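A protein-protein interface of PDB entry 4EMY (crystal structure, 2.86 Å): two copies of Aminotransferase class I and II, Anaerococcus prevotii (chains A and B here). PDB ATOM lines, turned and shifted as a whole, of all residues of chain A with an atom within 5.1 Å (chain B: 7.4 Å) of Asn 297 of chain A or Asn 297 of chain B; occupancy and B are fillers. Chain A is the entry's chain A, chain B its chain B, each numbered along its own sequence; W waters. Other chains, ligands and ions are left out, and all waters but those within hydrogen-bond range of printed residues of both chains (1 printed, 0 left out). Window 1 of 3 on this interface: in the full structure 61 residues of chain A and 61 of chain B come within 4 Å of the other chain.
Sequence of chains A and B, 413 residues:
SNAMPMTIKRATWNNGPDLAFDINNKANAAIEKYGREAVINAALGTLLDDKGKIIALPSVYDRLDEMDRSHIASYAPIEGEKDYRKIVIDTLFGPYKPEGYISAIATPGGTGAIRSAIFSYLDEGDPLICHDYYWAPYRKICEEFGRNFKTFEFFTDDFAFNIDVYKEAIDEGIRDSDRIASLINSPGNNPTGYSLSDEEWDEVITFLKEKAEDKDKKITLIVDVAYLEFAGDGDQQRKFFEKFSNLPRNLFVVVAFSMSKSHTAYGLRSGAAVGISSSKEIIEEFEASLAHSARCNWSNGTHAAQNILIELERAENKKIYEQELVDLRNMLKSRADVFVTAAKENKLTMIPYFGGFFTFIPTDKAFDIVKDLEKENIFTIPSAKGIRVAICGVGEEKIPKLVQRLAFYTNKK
Hydrophobic or aromatic side chains of chain B that line the printed part of chain A: Pro 108, Phe 119, Ile 141, Phe 145, His 292 and Trp 298.
Of the 13 printed residues of chain A, 12 touch a printed residue of chain B.
Among the printed residues, Asp or Glu carboxylates within 4 Å of a Lys or Arg side-chain nitrogen of the other chain: Glu 144 of chain A with Arg 115 of chain B.
Of chain A, only Pro 108 (3.9 Å), Gly 112 (3.7 Å), Arg 115 (2.9 Å), Glu 144 (3.5 Å), Phe 145 (3.6 Å) and Asn 297 (3.6 Å) come within 4 Å of Asn 297 of chain B.
Of the printed residues of chain B, Cys 296 of chain A touches Thr 111, Arg 115, Ile 141 and Glu 144.
Printed residues of chain A within 4 Å of Ser 299 of chain B: Thr 111.
The nearest residue of chain A that does not touch Asn 297 of chain B is Thr 111 of chain A (4.1 Å).
Arg 115 of chain A touches Asn 297 of chain B, and with the chains exchanged Asn 297 of chain A touches Arg 115 of chain B.
Phe 145 of chain A touches Asn 297 of chain B, and with the chains exchanged Asn 297 of chain A touches Phe 145 of chain B.
The side-chain hydroxyl (OG1) of Thr 111 of chain A lies within hydrogen-bond range of the side-chain hydroxyl (OG) of Ser 299 of chain B (3.3 Å).
The side-chain sulfur of Cys 296 of chain A lies within hydrogen-bond range of the backbone NH of Ile 141 of chain B (3.6 Å).
The side-chain amide oxygen of Asn 297 of chain A sits at hydrogen-bond distance from the guanidinium group of Arg 115 of chain B, 2.9 Å away.
The side-chain hydroxyl (OG) of Ser 293 of chain B is in hydrogen-bond range of the side-chain carboxylate (OE2) of Glu 144 of chain A, 2.7 Å away.
OG of Ser 293 of chain A lies within hydrogen-bond range of OE2 of Glu 144 of chain B (2.6 Å).
The guanidinium group (NH1) of Arg 115 of chain B is in salt-bridge range of the side-chain carboxylate (OE2) of Glu 144 of chain A (3.5 Å).
The guanidinium group of Arg 269 of chain B sits at hydrogen-bond distance from the backbone carbonyl oxygen of Trp 298 of chain A (3.1 Å).
OE2 of Glu 144 of chain A sits at hydrogen-bond distance from ND2 of Asn 297 of chain B, 3.5 Å away.
A ring nitrogen (ND1) of His 292 of chain B sits at hydrogen-bond distance from the side-chain carboxylate (OE1) of Glu 144 of chain A (2.8 Å).
The guanidinium group (NE) of Arg 115 of chain A lies within hydrogen-bond range of the side-chain amide oxygen (OD1) of Asn 297 of chain B.
The backbone carbonyl oxygen (O) of Arg 269 of chain B sits close to the backbone NH (N) of Gly 109 of chain B (3.5 Å).
O of Pro 108 of chain B sits at hydrogen-bond distance from NH2 of Arg 269 of chain B, at 3.5 Å.
Water W1 lies within hydrogen-bond range of the guanidinium group of Arg 115 of chain A (2.5 Å), the side-chain carboxylate of Glu 144 of chain B (2.7 Å) and the side-chain amide nitrogen of Asn 297 of chain A (3.2 Å).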
ATOM      1  N   PRO A 108       3.586 -12.499  12.146  1.00  0.00           N
ATOM      2  CA  PRO A 108       4.078 -12.145  10.811  1.00  0.00           C
ATOM      3  C   PRO A 108       4.203 -13.417   9.965  1.00  0.00           C
ATOM      4  O   PRO A 108       5.200 -14.149  10.058  1.00  0.00           O
ATOM      5  CB  PRO A 108       5.431 -11.483  11.093  1.00  0.00           C
ATOM      6  CG  PRO A 108       5.871 -12.039  12.410  1.00  0.00           C
ATOM      7  CD  PRO A 108       4.640 -12.425  13.178  1.00  0.00           C
ATOM      8  N   THR A 111       5.530 -18.175   9.663  1.00  0.00           N
ATOM      9  CA  THR A 111       6.825 -18.132  10.330  1.00  0.00           C
ATOM     10  C   THR A 111       6.670 -17.605  11.759  1.00  0.00           C
ATOM     11  O   THR A 111       7.195 -18.203  12.718  1.00  0.00           O
ATOM     12  CB  THR A 111       7.837 -17.279   9.533  1.00  0.00           C
ATOM     13  OG1 THR A 111       8.011 -17.834   8.222  1.00  0.00           O
ATOM     14  CG2 THR A 111       9.191 -17.225  10.236  1.00  0.00           C
ATOM     15  N   GLY A 112       5.925 -16.505  11.893  1.00  0.00           N
ATOM     16  CA  GLY A 112       5.637 -15.909  13.192  1.00  0.00           C
ATOM     17  C   GLY A 112       5.037 -16.900  14.175  1.00  0.00           C
ATOM     18  O   GLY A 112       5.458 -16.976  15.332  1.00  0.00           O
ATOM     19  N   ARG A 115       7.786 -19.974  15.251  1.00  0.00           N
ATOM     20  CA  ARG A 115       8.854 -19.592  16.181  1.00  0.00           C
ATOM     21  C   ARG A 115       8.302 -19.369  17.586  1.00  0.00           C
ATOM     22  O   ARG A 115       8.964 -19.676  18.583  1.00  0.00           O
ATOM     23  CB  ARG A 115       9.581 -18.323  15.711  1.00  0.00           C
ATOM     24  CG  ARG A 115       8.725 -17.062  15.751  1.00  0.00           C
ATOM     25  CD  ARG A 115       9.497 -15.808  16.150  1.00  0.00           C
ATOM     26  NE  ARG A 115       9.970 -15.792  17.541  1.00  0.00           N
ATOM     27  CZ  ARG A 115       9.216 -15.497  18.601  1.00  0.00           C
ATOM     28  NH1 ARG A 115       9.744 -15.509  19.819  1.00  0.00           N
ATOM     29  NH2 ARG A 115       7.929 -15.207  18.454  1.00  0.00           N
ATOM     30  N   GLU A 144      18.600 -20.861  16.723  1.00  0.00           N
ATOM     31  CA  GLU A 144      18.560 -19.475  17.179  1.00  0.00           C
ATOM     32  C   GLU A 144      18.251 -19.440  18.678  1.00  0.00           C
ATOM     33  O   GLU A 144      18.942 -18.767  19.443  1.00  0.00           O
ATOM     34  CB  GLU A 144      17.532 -18.665  16.369  1.00  0.00           C
ATOM     35  CG  GLU A 144      17.288 -17.239  16.863  1.00  0.00           C
ATOM     36  CD  GLU A 144      17.795 -16.139  15.929  1.00  0.00           C
ATOM     37  OE1 GLU A 144      18.721 -16.378  15.117  1.00  0.00           O
ATOM     38  OE2 GLU A 144      17.260 -15.011  16.022  1.00  0.00           O
ATOM     39  N   PHE A 145      17.237 -20.197  19.088  1.00  0.00           N
ATOM     40  CA  PHE A 145      16.758 -20.173  20.465  1.00  0.00           C
ATOM     41  C   PHE A 145      17.321 -21.286  21.343  1.00  0.00           C
ATOM     42  O   PHE A 145      16.939 -21.412  22.507  1.00  0.00           O
ATOM     43  CB  PHE A 145      15.228 -20.182  20.509  1.00  0.00           C
ATOM     44  CG  PHE A 145      14.597 -19.017  19.806  1.00  0.00           C
ATOM     45  CD1 PHE A 145      15.078 -17.727  19.994  1.00  0.00           C
ATOM     46  CD2 PHE A 145      13.512 -19.208  18.962  1.00  0.00           C
ATOM     47  CE1 PHE A 145      14.497 -16.654  19.336  1.00  0.00           C
ATOM     48  CE2 PHE A 145      12.922 -18.140  18.310  1.00  0.00           C
ATOM     49  CZ  PHE A 145      13.413 -16.862  18.498  1.00  0.00           C
ATOM     50  N   SER A 293       5.300 -12.050  23.522  1.00  0.00           N
ATOM     51  CA  SER A 293       6.225 -12.309  22.422  1.00  0.00           C
ATOM     52  C   SER A 293       5.999 -11.345  21.257  1.00  0.00           C
ATOM     53  O   SER A 293       6.965 -10.806  20.716  1.00  0.00           O
ATOM     54  CB  SER A 293       6.124 -13.761  21.937  1.00  0.00           C
ATOM     55  OG  SER A 293       6.956 -14.631  22.683  1.00  0.00           O
ATOM     56  N   ALA A 294       4.736 -11.124  20.881  1.00  0.00           N
ATOM     57  CA  ALA A 294       4.409 -10.210  19.766  1.00  0.00           C
ATOM     58  C   ALA A 294       4.919  -8.812  20.056  1.00  0.00           C
ATOM     59  O   ALA A 294       5.437  -8.137  19.164  1.00  0.00           O
ATOM     60  CB  ALA A 294       2.910 -10.169  19.494  1.00  0.00           C
ATOM     61  N   ARG A 295       4.790  -8.401  21.317  1.00  0.00           N
ATOM     62  CA  ARG A 295       5.152  -7.056  21.726  1.00  0.00           C
ATOM     63  C   ARG A 295       6.646  -6.851  21.647  1.00  0.00           C
ATOM     64  O   ARG A 295       7.111  -5.761  21.328  1.00  0.00           O
ATOM     65  CB  ARG A 295       4.663  -6.743  23.143  1.00  0.00           C
ATOM     66  CG  ARG A 295       4.592  -5.246  23.403  1.00  0.00           C
ATOM     67  CD  ARG A 295       3.801  -4.571  22.274  1.00  0.00           C
ATOM     68  NE  ARG A 295       4.172  -3.182  21.987  1.00  0.00           N
ATOM     69  CZ  ARG A 295       4.015  -2.159  22.824  1.00  0.00           C
ATOM     70  NH1 ARG A 295       3.525  -2.344  24.048  1.00  0.00           N
ATOM     71  NH2 ARG A 295       4.373  -0.940  22.439  1.00  0.00           N
ATOM     72  N   CYS A 296       7.382  -7.918  21.915  1.00  0.00           N
ATOM     73  CA  CYS A 296       8.823  -7.866  21.935  1.00  0.00           C
ATOM     74  C   CYS A 296       9.443  -8.067  20.569  1.00  0.00           C
ATOM     75  O   CYS A 296      10.458  -7.463  20.259  1.00  0.00           O
ATOM     76  CB  CYS A 296       9.361  -8.888  22.929  1.00  0.00           C
ATOM     77  SG  CYS A 296       8.846  -8.513  24.621  1.00  0.00           S
ATOM     78  N   ASN A 297       8.823  -8.893  19.738  1.00  0.00           N
ATOM     79  CA  ASN A 297       9.433  -9.264  18.468  1.00  0.00           C
ATOM     80  C   ASN A 297       8.990  -8.468  17.232  1.00  0.00           C
ATOM     81  O   ASN A 297       9.828  -8.128  16.403  1.00  0.00           O
ATOM     82  CB  ASN A 297       9.329 -10.779  18.249  1.00  0.00           C
ATOM     83  CG  ASN A 297      10.085 -11.572  19.312  1.00  0.00           C
ATOM     84  OD1 ASN A 297      11.319 -11.599  19.319  1.00  0.00           O
ATOM     85  ND2 ASN A 297       9.351 -12.211  20.218  1.00  0.00           N
ATOM     86  N   TRP A 298       7.703  -8.153  17.109  1.00  0.00           N
ATOM     87  CA  TRP A 298       7.224  -7.404  15.933  1.00  0.00           C
ATOM     88  C   TRP A 298       6.225  -6.313  16.239  1.00  0.00           C
ATOM     89  O   TRP A 298       5.749  -5.623  15.333  1.00  0.00           O
ATOM     90  CB  TRP A 298       6.669  -8.356  14.876  1.00  0.00           C
ATOM     91  CG  TRP A 298       5.543  -9.222  15.376  1.00  0.00           C
ATOM     92  CD1 TRP A 298       4.192  -8.898  15.455  1.00  0.00           C
ATOM     93  CD2 TRP A 298       5.636 -10.597  15.890  1.00  0.00           C
ATOM     94  NE1 TRP A 298       3.466  -9.945  15.970  1.00  0.00           N
ATOM     95  CE2 TRP A 298       4.271 -10.993  16.251  1.00  0.00           C
ATOM     96  CE3 TRP A 298       6.673 -11.504  16.075  1.00  0.00           C
ATOM     97  CZ2 TRP A 298       3.984 -12.246  16.767  1.00  0.00           C
ATOM     98  CZ3 TRP A 298       6.372 -12.762  16.601  1.00  0.00           C
ATOM     99  CH2 TRP A 298       5.059 -13.123  16.937  1.00  0.00           C
ATOM    100  N   SER A 299       5.912  -6.153  17.525  1.00  0.00           N
ATOM    101  CA  SER A 299       4.926  -5.178  18.028  1.00  0.00           C
ATOM    102  C   SER A 299       3.473  -5.467  17.634  1.00  0.00           C
ATOM    103  O   SER A 299       2.601  -5.531  18.491  1.00  0.00           O
ATOM    104  CB  SER A 299       5.314  -3.742  17.669  1.00  0.00           C
ATOM    105  OG  SER A 299       4.498  -2.825  18.362  1.00  0.00           O
ATOM    106  N   THR B 107      13.435  -4.790   9.108  1.00  0.00           N
ATOM    107  CA  THR B 107      12.797  -5.338  10.305  1.00  0.00           C
ATOM    108  C   THR B 107      11.315  -4.928  10.357  1.00  0.00           C
ATOM    109  O   THR B 107      10.906  -4.013   9.635  1.00  0.00           O
ATOM    110  CB  THR B 107      13.484  -4.823  11.588  1.00  0.00           C
ATOM    111  OG1 THR B 107      13.585  -3.395  11.541  1.00  0.00           O
ATOM    112  CG2 THR B 107      14.873  -5.425  11.760  1.00  0.00           C
ATOM    113  N   PRO B 108      10.503  -5.595  11.213  1.00  0.00           N
ATOM    114  CA  PRO B 108       9.132  -5.126  11.378  1.00  0.00           C
ATOM    115  C   PRO B 108       9.129  -3.889  12.274  1.00  0.00           C
ATOM    116  O   PRO B 108       9.173  -4.003  13.508  1.00  0.00           O
ATOM    117  CB  PRO B 108       8.422  -6.307  12.062  1.00  0.00           C
ATOM    118  CG  PRO B 108       9.448  -7.374  12.245  1.00  0.00           C
ATOM    119  CD  PRO B 108      10.788  -6.729  12.104  1.00  0.00           C
ATOM    120  N   GLY B 109       9.121  -2.716  11.637  1.00  0.00           N
ATOM    121  CA  GLY B 109       9.194  -1.440  12.343  1.00  0.00           C
ATOM    122  C   GLY B 109      10.465  -1.294  13.158  1.00  0.00           C
ATOM    123  O   GLY B 109      11.354  -2.149  13.097  1.00  0.00           O
ATOM    124  N   GLY B 110      10.554  -0.204  13.917  1.00  0.00           N
ATOM    125  CA  GLY B 110      11.683   0.029  14.811  1.00  0.00           C
ATOM    126  C   GLY B 110      11.833  -1.055  15.869  1.00  0.00           C
ATOM    127  O   GLY B 110      12.953  -1.414  16.241  1.00  0.00           O
ATOM    128  N   THR B 111      10.694  -1.578  16.329  1.00  0.00           N
ATOM    129  CA  THR B 111      10.634  -2.677  17.289  1.00  0.00           C
ATOM    130  C   THR B 111      11.522  -3.857  16.885  1.00  0.00           C
ATOM    131  O   THR B 111      12.277  -4.384  17.709  1.00  0.00           O
ATOM    132  CB  THR B 111       9.180  -3.141  17.500  1.00  0.00           C
ATOM    133  OG1 THR B 111       8.385  -2.011  17.873  1.00  0.00           O
ATOM    134  CG2 THR B 111       9.076  -4.196  18.593  1.00  0.00           C
ATOM    135  N   GLY B 112      11.444  -4.249  15.617  1.00  0.00           N
ATOM    136  CA  GLY B 112      12.220  -5.380  15.125  1.00  0.00           C
ATOM    137  C   GLY B 112      13.705  -5.115  15.245  1.00  0.00           C
ATOM    138  O   GLY B 112      14.474  -5.990  15.663  1.00  0.00           O
ATOM    139  N   ALA B 113      14.095  -3.892  14.892  1.00  0.00           N
ATOM    140  CA  ALA B 113      15.479  -3.461  14.971  1.00  0.00           C
ATOM    141  C   ALA B 113      15.995  -3.475  16.418  1.00  0.00           C
ATOM    142  O   ALA B 113      17.115  -3.919  16.682  1.00  0.00           O
ATOM    143  CB  ALA B 113      15.623  -2.084  14.360  1.00  0.00           C
ATOM    144  N   ARG B 115      14.723  -5.115  19.242  1.00  0.00           N
ATOM    145  CA  ARG B 115      14.760  -6.522  19.601  1.00  0.00           C
ATOM    146  C   ARG B 115      16.071  -7.174  19.154  1.00  0.00           C
ATOM    147  O   ARG B 115      16.811  -7.742  19.970  1.00  0.00           O
ATOM    148  CB  ARG B 115      13.585  -7.232  18.927  1.00  0.00           C
ATOM    149  CG  ARG B 115      13.624  -8.739  19.054  1.00  0.00           C
ATOM    150  CD  ARG B 115      13.400  -9.447  17.723  1.00  0.00           C
ATOM    151  NE  ARG B 115      13.733 -10.873  17.846  1.00  0.00           N
ATOM    152  CZ  ARG B 115      14.899 -11.414  17.487  1.00  0.00           C
ATOM    153  NH1 ARG B 115      15.112 -12.718  17.645  1.00  0.00           N
ATOM    154  NH2 ARG B 115      15.853 -10.655  16.959  1.00  0.00           N
ATOM    155  N   SER B 116      16.350  -7.073  17.853  1.00  0.00           N
ATOM    156  CA  SER B 116      17.489  -7.745  17.238  1.00  0.00           C
ATOM    157  C   SER B 116      18.837  -7.326  17.821  1.00  0.00           C
ATOM    158  O   SER B 116      19.698  -8.172  18.073  1.00  0.00           O
ATOM    159  CB  SER B 116      17.462  -7.548  15.724  1.00  0.00           C
ATOM    160  OG  SER B 116      16.338  -8.194  15.148  1.00  0.00           O
ATOM    161  N   PHE B 119      19.130  -8.857  21.215  1.00  0.00           N
ATOM    162  CA  PHE B 119      19.350 -10.289  21.103  1.00  0.00           C
ATOM    163  C   PHE B 119      20.788 -10.616  20.719  1.00  0.00           C
ATOM    164  O   PHE B 119      21.430 -11.453  21.358  1.00  0.00           O
ATOM    165  CB  PHE B 119      18.395 -10.904  20.091  1.00  0.00           C
ATOM    166  CG  PHE B 119      18.496 -12.394  20.005  1.00  0.00           C
ATOM    167  CD1 PHE B 119      18.945 -13.007  18.840  1.00  0.00           C
ATOM    168  CD2 PHE B 119      18.158 -13.192  21.099  1.00  0.00           C
ATOM    169  CE1 PHE B 119      19.042 -14.388  18.763  1.00  0.00           C
ATOM    170  CE2 PHE B 119      18.254 -14.571  21.026  1.00  0.00           C
ATOM    171  CZ  PHE B 119      18.697 -15.169  19.857  1.00  0.00           C
ATOM    172  N   ILE B 141      11.512  -6.733  26.293  1.00  0.00           N
ATOM    173  CA  ILE B 141      12.384  -7.502  25.409  1.00  0.00           C
ATOM    174  C   ILE B 141      13.489  -8.175  26.220  1.00  0.00           C
ATOM    175  O   ILE B 141      13.681  -9.386  26.115  1.00  0.00           O
ATOM    176  CB  ILE B 141      12.946  -6.643  24.253  1.00  0.00           C
ATOM    177  CG1 ILE B 141      11.826  -6.293  23.282  1.00  0.00           C
ATOM    178  CG2 ILE B 141      14.049  -7.374  23.500  1.00  0.00           C
ATOM    179  CD1 ILE B 141      12.189  -5.216  22.290  1.00  0.00           C
ATOM    180  N   GLU B 144      11.953 -10.989  28.028  1.00  0.00           N
ATOM    181  CA  GLU B 144      11.660 -12.031  27.037  1.00  0.00           C
ATOM    182  C   GLU B 144      12.884 -12.896  26.728  1.00  0.00           C
ATOM    183  O   GLU B 144      12.762 -14.106  26.568  1.00  0.00           O
ATOM    184  CB  GLU B 144      11.159 -11.370  25.743  1.00  0.00           C
ATOM    185  CG  GLU B 144      10.915 -12.304  24.563  1.00  0.00           C
ATOM    186  CD  GLU B 144       9.495 -12.838  24.493  1.00  0.00           C
ATOM    187  OE1 GLU B 144       8.690 -12.559  25.410  1.00  0.00           O
ATOM    188  OE2 GLU B 144       9.181 -13.544  23.510  1.00  0.00           O
ATOM    189  N   PHE B 145      14.056 -12.270  26.637  1.00  0.00           N
ATOM    190  CA  PHE B 145      15.281 -12.972  26.269  1.00  0.00           C
ATOM    191  C   PHE B 145      16.249 -13.143  27.430  1.00  0.00           C
ATOM    192  O   PHE B 145      17.407 -13.491  27.217  1.00  0.00           O
ATOM    193  CB  PHE B 145      15.997 -12.247  25.129  1.00  0.00           C
ATOM    194  CG  PHE B 145      15.186 -12.130  23.867  1.00  0.00           C
ATOM    195  CD1 PHE B 145      14.679 -13.263  23.235  1.00  0.00           C
ATOM    196  CD2 PHE B 145      14.953 -10.888  23.295  1.00  0.00           C
ATOM    197  CE1 PHE B 145      13.941 -13.157  22.068  1.00  0.00           C
ATOM    198  CE2 PHE B 145      14.223 -10.775  22.129  1.00  0.00           C
ATOM    199  CZ  PHE B 145      13.717 -11.911  21.516  1.00  0.00           C
ATOM    200  N   ARG B 269       4.378  -1.848   9.378  1.00  0.00           N
ATOM    201  CA  ARG B 269       5.448  -2.557  10.094  1.00  0.00           C
ATOM    202  C   ARG B 269       6.752  -2.640   9.298  1.00  0.00           C
ATOM    203  O   ARG B 269       7.193  -3.726   8.900  1.00  0.00           O
ATOM    204  CB  ARG B 269       4.976  -3.950  10.508  1.00  0.00           C
ATOM    205  CG  ARG B 269       3.562  -3.998  11.071  1.00  0.00           C
ATOM    206  CD  ARG B 269       3.391  -3.121  12.302  1.00  0.00           C
ATOM    207  NE  ARG B 269       4.451  -3.313  13.298  1.00  0.00           N
ATOM    208  CZ  ARG B 269       5.275  -2.353  13.720  1.00  0.00           C
ATOM    209  NH1 ARG B 269       5.175  -1.111  13.260  1.00  0.00           N
ATOM    210  NH2 ARG B 269       6.204  -2.632  14.621  1.00  0.00           N
ATOM    211  N   ALA B 291      20.351 -11.421   9.465  1.00  0.00           N
ATOM    212  CA  ALA B 291      19.728 -12.158   8.369  1.00  0.00           C
ATOM    213  C   ALA B 291      19.133 -13.448   8.900  1.00  0.00           C
ATOM    214  O   ALA B 291      18.035 -13.832   8.513  1.00  0.00           O
ATOM    215  CB  ALA B 291      20.728 -12.447   7.266  1.00  0.00           C
ATOM    216  N   HIS B 292      19.858 -14.102   9.805  1.00  0.00           N
ATOM    217  CA  HIS B 292      19.395 -15.346  10.416  1.00  0.00           C
ATOM    218  C   HIS B 292      18.198 -15.097  11.286  1.00  0.00           C
ATOM    219  O   HIS B 292      17.213 -15.821  11.214  1.00  0.00           O
ATOM    220  CB  HIS B 292      20.518 -15.999  11.212  1.00  0.00           C
ATOM    221  CG  HIS B 292      20.218 -17.412  11.646  1.00  0.00           C
ATOM    222  ND1 HIS B 292      19.494 -17.693  12.744  1.00  0.00           N
ATOM    223  CD2 HIS B 292      20.579 -18.634  11.090  1.00  0.00           C
ATOM    224  CE1 HIS B 292      19.386 -19.026  12.881  1.00  0.00           C
ATOM    225  NE2 HIS B 292      20.053 -19.602  11.869  1.00  0.00           N
ATOM    226  N   SER B 293      18.272 -14.057  12.107  1.00  0.00           N
ATOM    227  CA  SER B 293      17.175 -13.692  13.003  1.00  0.00           C
ATOM    228  C   SER B 293      15.911 -13.304  12.251  1.00  0.00           C
ATOM    229  O   SER B 293      14.812 -13.703  12.640  1.00  0.00           O
ATOM    230  CB  SER B 293      17.597 -12.567  13.944  1.00  0.00           C
ATOM    231  OG  SER B 293      18.634 -13.019  14.789  1.00  0.00           O
ATOM    232  N   ALA B 294      16.070 -12.526  11.182  1.00  0.00           N
ATOM    233  CA  ALA B 294      14.944 -12.174  10.326  1.00  0.00           C
ATOM    234  C   ALA B 294      14.286 -13.448   9.810  1.00  0.00           C
ATOM    235  O   ALA B 294      13.066 -13.604   9.886  1.00  0.00           O
ATOM    236  CB  ALA B 294      15.394 -11.295   9.172  1.00  0.00           C
ATOM    237  N   ARG B 295      15.106 -14.374   9.326  1.00  0.00           N
ATOM    238  CA  ARG B 295      14.604 -15.616   8.777  1.00  0.00           C
ATOM    239  C   ARG B 295      13.861 -16.458   9.821  1.00  0.00           C
ATOM    240  O   ARG B 295      12.968 -17.231   9.475  1.00  0.00           O
ATOM    241  CB  ARG B 295      15.741 -16.424   8.135  1.00  0.00           C
ATOM    242  CG  ARG B 295      15.241 -17.528   7.207  1.00  0.00           C
ATOM    243  CD  ARG B 295      14.252 -16.953   6.196  1.00  0.00           C
ATOM    244  NE  ARG B 295      13.264 -17.905   5.691  1.00  0.00           N
ATOM    245  CZ  ARG B 295      13.508 -18.819   4.755  1.00  0.00           C
ATOM    246  NH1 ARG B 295      14.725 -18.938   4.233  1.00  0.00           N
ATOM    247  NH2 ARG B 295      12.538 -19.628   4.344  1.00  0.00           N
ATOM    248  N   CYS B 296      14.218 -16.294  11.090  1.00  0.00           N
ATOM    249  CA  CYS B 296      13.658 -17.125  12.148  1.00  0.00           C
ATOM    250  C   CYS B 296      12.490 -16.501  12.892  1.00  0.00           C
ATOM    251  O   CYS B 296      11.736 -17.211  13.570  1.00  0.00           O
ATOM    252  CB  CYS B 296      14.741 -17.498  13.151  1.00  0.00           C
ATOM    253  SG  CYS B 296      16.016 -18.517  12.410  1.00  0.00           S
ATOM    254  N   ASN B 297      12.340 -15.186  12.790  1.00  0.00           N
ATOM    255  CA  ASN B 297      11.320 -14.512  13.572  1.00  0.00           C
ATOM    256  C   ASN B 297      10.135 -14.021  12.756  1.00  0.00           C
ATOM    257  O   ASN B 297       8.994 -14.327  13.102  1.00  0.00           O
ATOM    258  CB  ASN B 297      11.928 -13.424  14.465  1.00  0.00           C
ATOM    259  CG  ASN B 297      12.675 -14.005  15.656  1.00  0.00           C
ATOM    260  OD1 ASN B 297      12.165 -14.018  16.776  1.00  0.00           O
ATOM    261  ND2 ASN B 297      13.880 -14.511  15.419  1.00  0.00           N
ATOM    262  N   TRP B 298      10.401 -13.286  11.675  1.00  0.00           N
ATOM    263  CA  TRP B 298       9.335 -12.761  10.812  1.00  0.00           C
ATOM    264  C   TRP B 298       9.434 -13.216   9.387  1.00  0.00           C
ATOM    265  O   TRP B 298       8.489 -13.055   8.617  1.00  0.00           O
ATOM    266  CB  TRP B 298       9.293 -11.240  10.856  1.00  0.00           C
ATOM    267  CG  TRP B 298      10.628 -10.582  10.606  1.00  0.00           C
ATOM    268  CD1 TRP B 298      11.203 -10.252   9.379  1.00  0.00           C
ATOM    269  CD2 TRP B 298      11.602 -10.140  11.615  1.00  0.00           C
ATOM    270  NE1 TRP B 298      12.427  -9.653   9.555  1.00  0.00           N
ATOM    271  CE2 TRP B 298      12.727  -9.555  10.872  1.00  0.00           C
ATOM    272  CE3 TRP B 298      11.648 -10.156  13.004  1.00  0.00           C
ATOM    273  CZ2 TRP B 298      13.837  -9.030  11.516  1.00  0.00           C
ATOM    274  CZ3 TRP B 298      12.770  -9.624  13.638  1.00  0.00           C
ATOM    275  CH2 TRP B 298      13.837  -9.075  12.911  1.00  0.00           C
ATOM    276  N   SER B 299      10.589 -13.778   9.033  1.00  0.00           N
ATOM    277  CA  SER B 299      10.868 -14.333   7.695  1.00  0.00           C
ATOM    278  C   SER B 299      11.424 -13.273   6.759  1.00  0.00           C
ATOM    279  O   SER B 299      12.535 -13.417   6.251  1.00  0.00           O
ATOM    280  CB  SER B 299       9.633 -15.004   7.081  1.00  0.00           C
ATOM    281  OG  SER B 299      10.002 -16.074   6.236  1.00  0.00           O
ATOM    282  N   ASN B 300      10.639 -12.215   6.551  1.00  0.00           N
ATOM    283  CA  ASN B 300      10.946 -11.110   5.633  1.00  0.00           C
ATOM    284  C   ASN B 300       9.933  -9.998   5.834  1.00  0.00           C
ATOM    285  O   ASN B 300       8.808 -10.256   6.249  1.00  0.00           O
ATOM    286  CB  ASN B 300      10.939 -11.565   4.175  1.00  0.00           C
ATOM    287  CG  ASN B 300       9.923 -12.659   3.908  1.00  0.00           C
ATOM    288  OD1 ASN B 300       8.745 -12.386   3.712  1.00  0.00           O
ATOM    289  ND2 ASN B 300      10.382 -13.911   3.901  1.00  0.00           N
HETATM  290  O   HOH W   1      10.978 -14.437  21.745  1.00  0.00           O
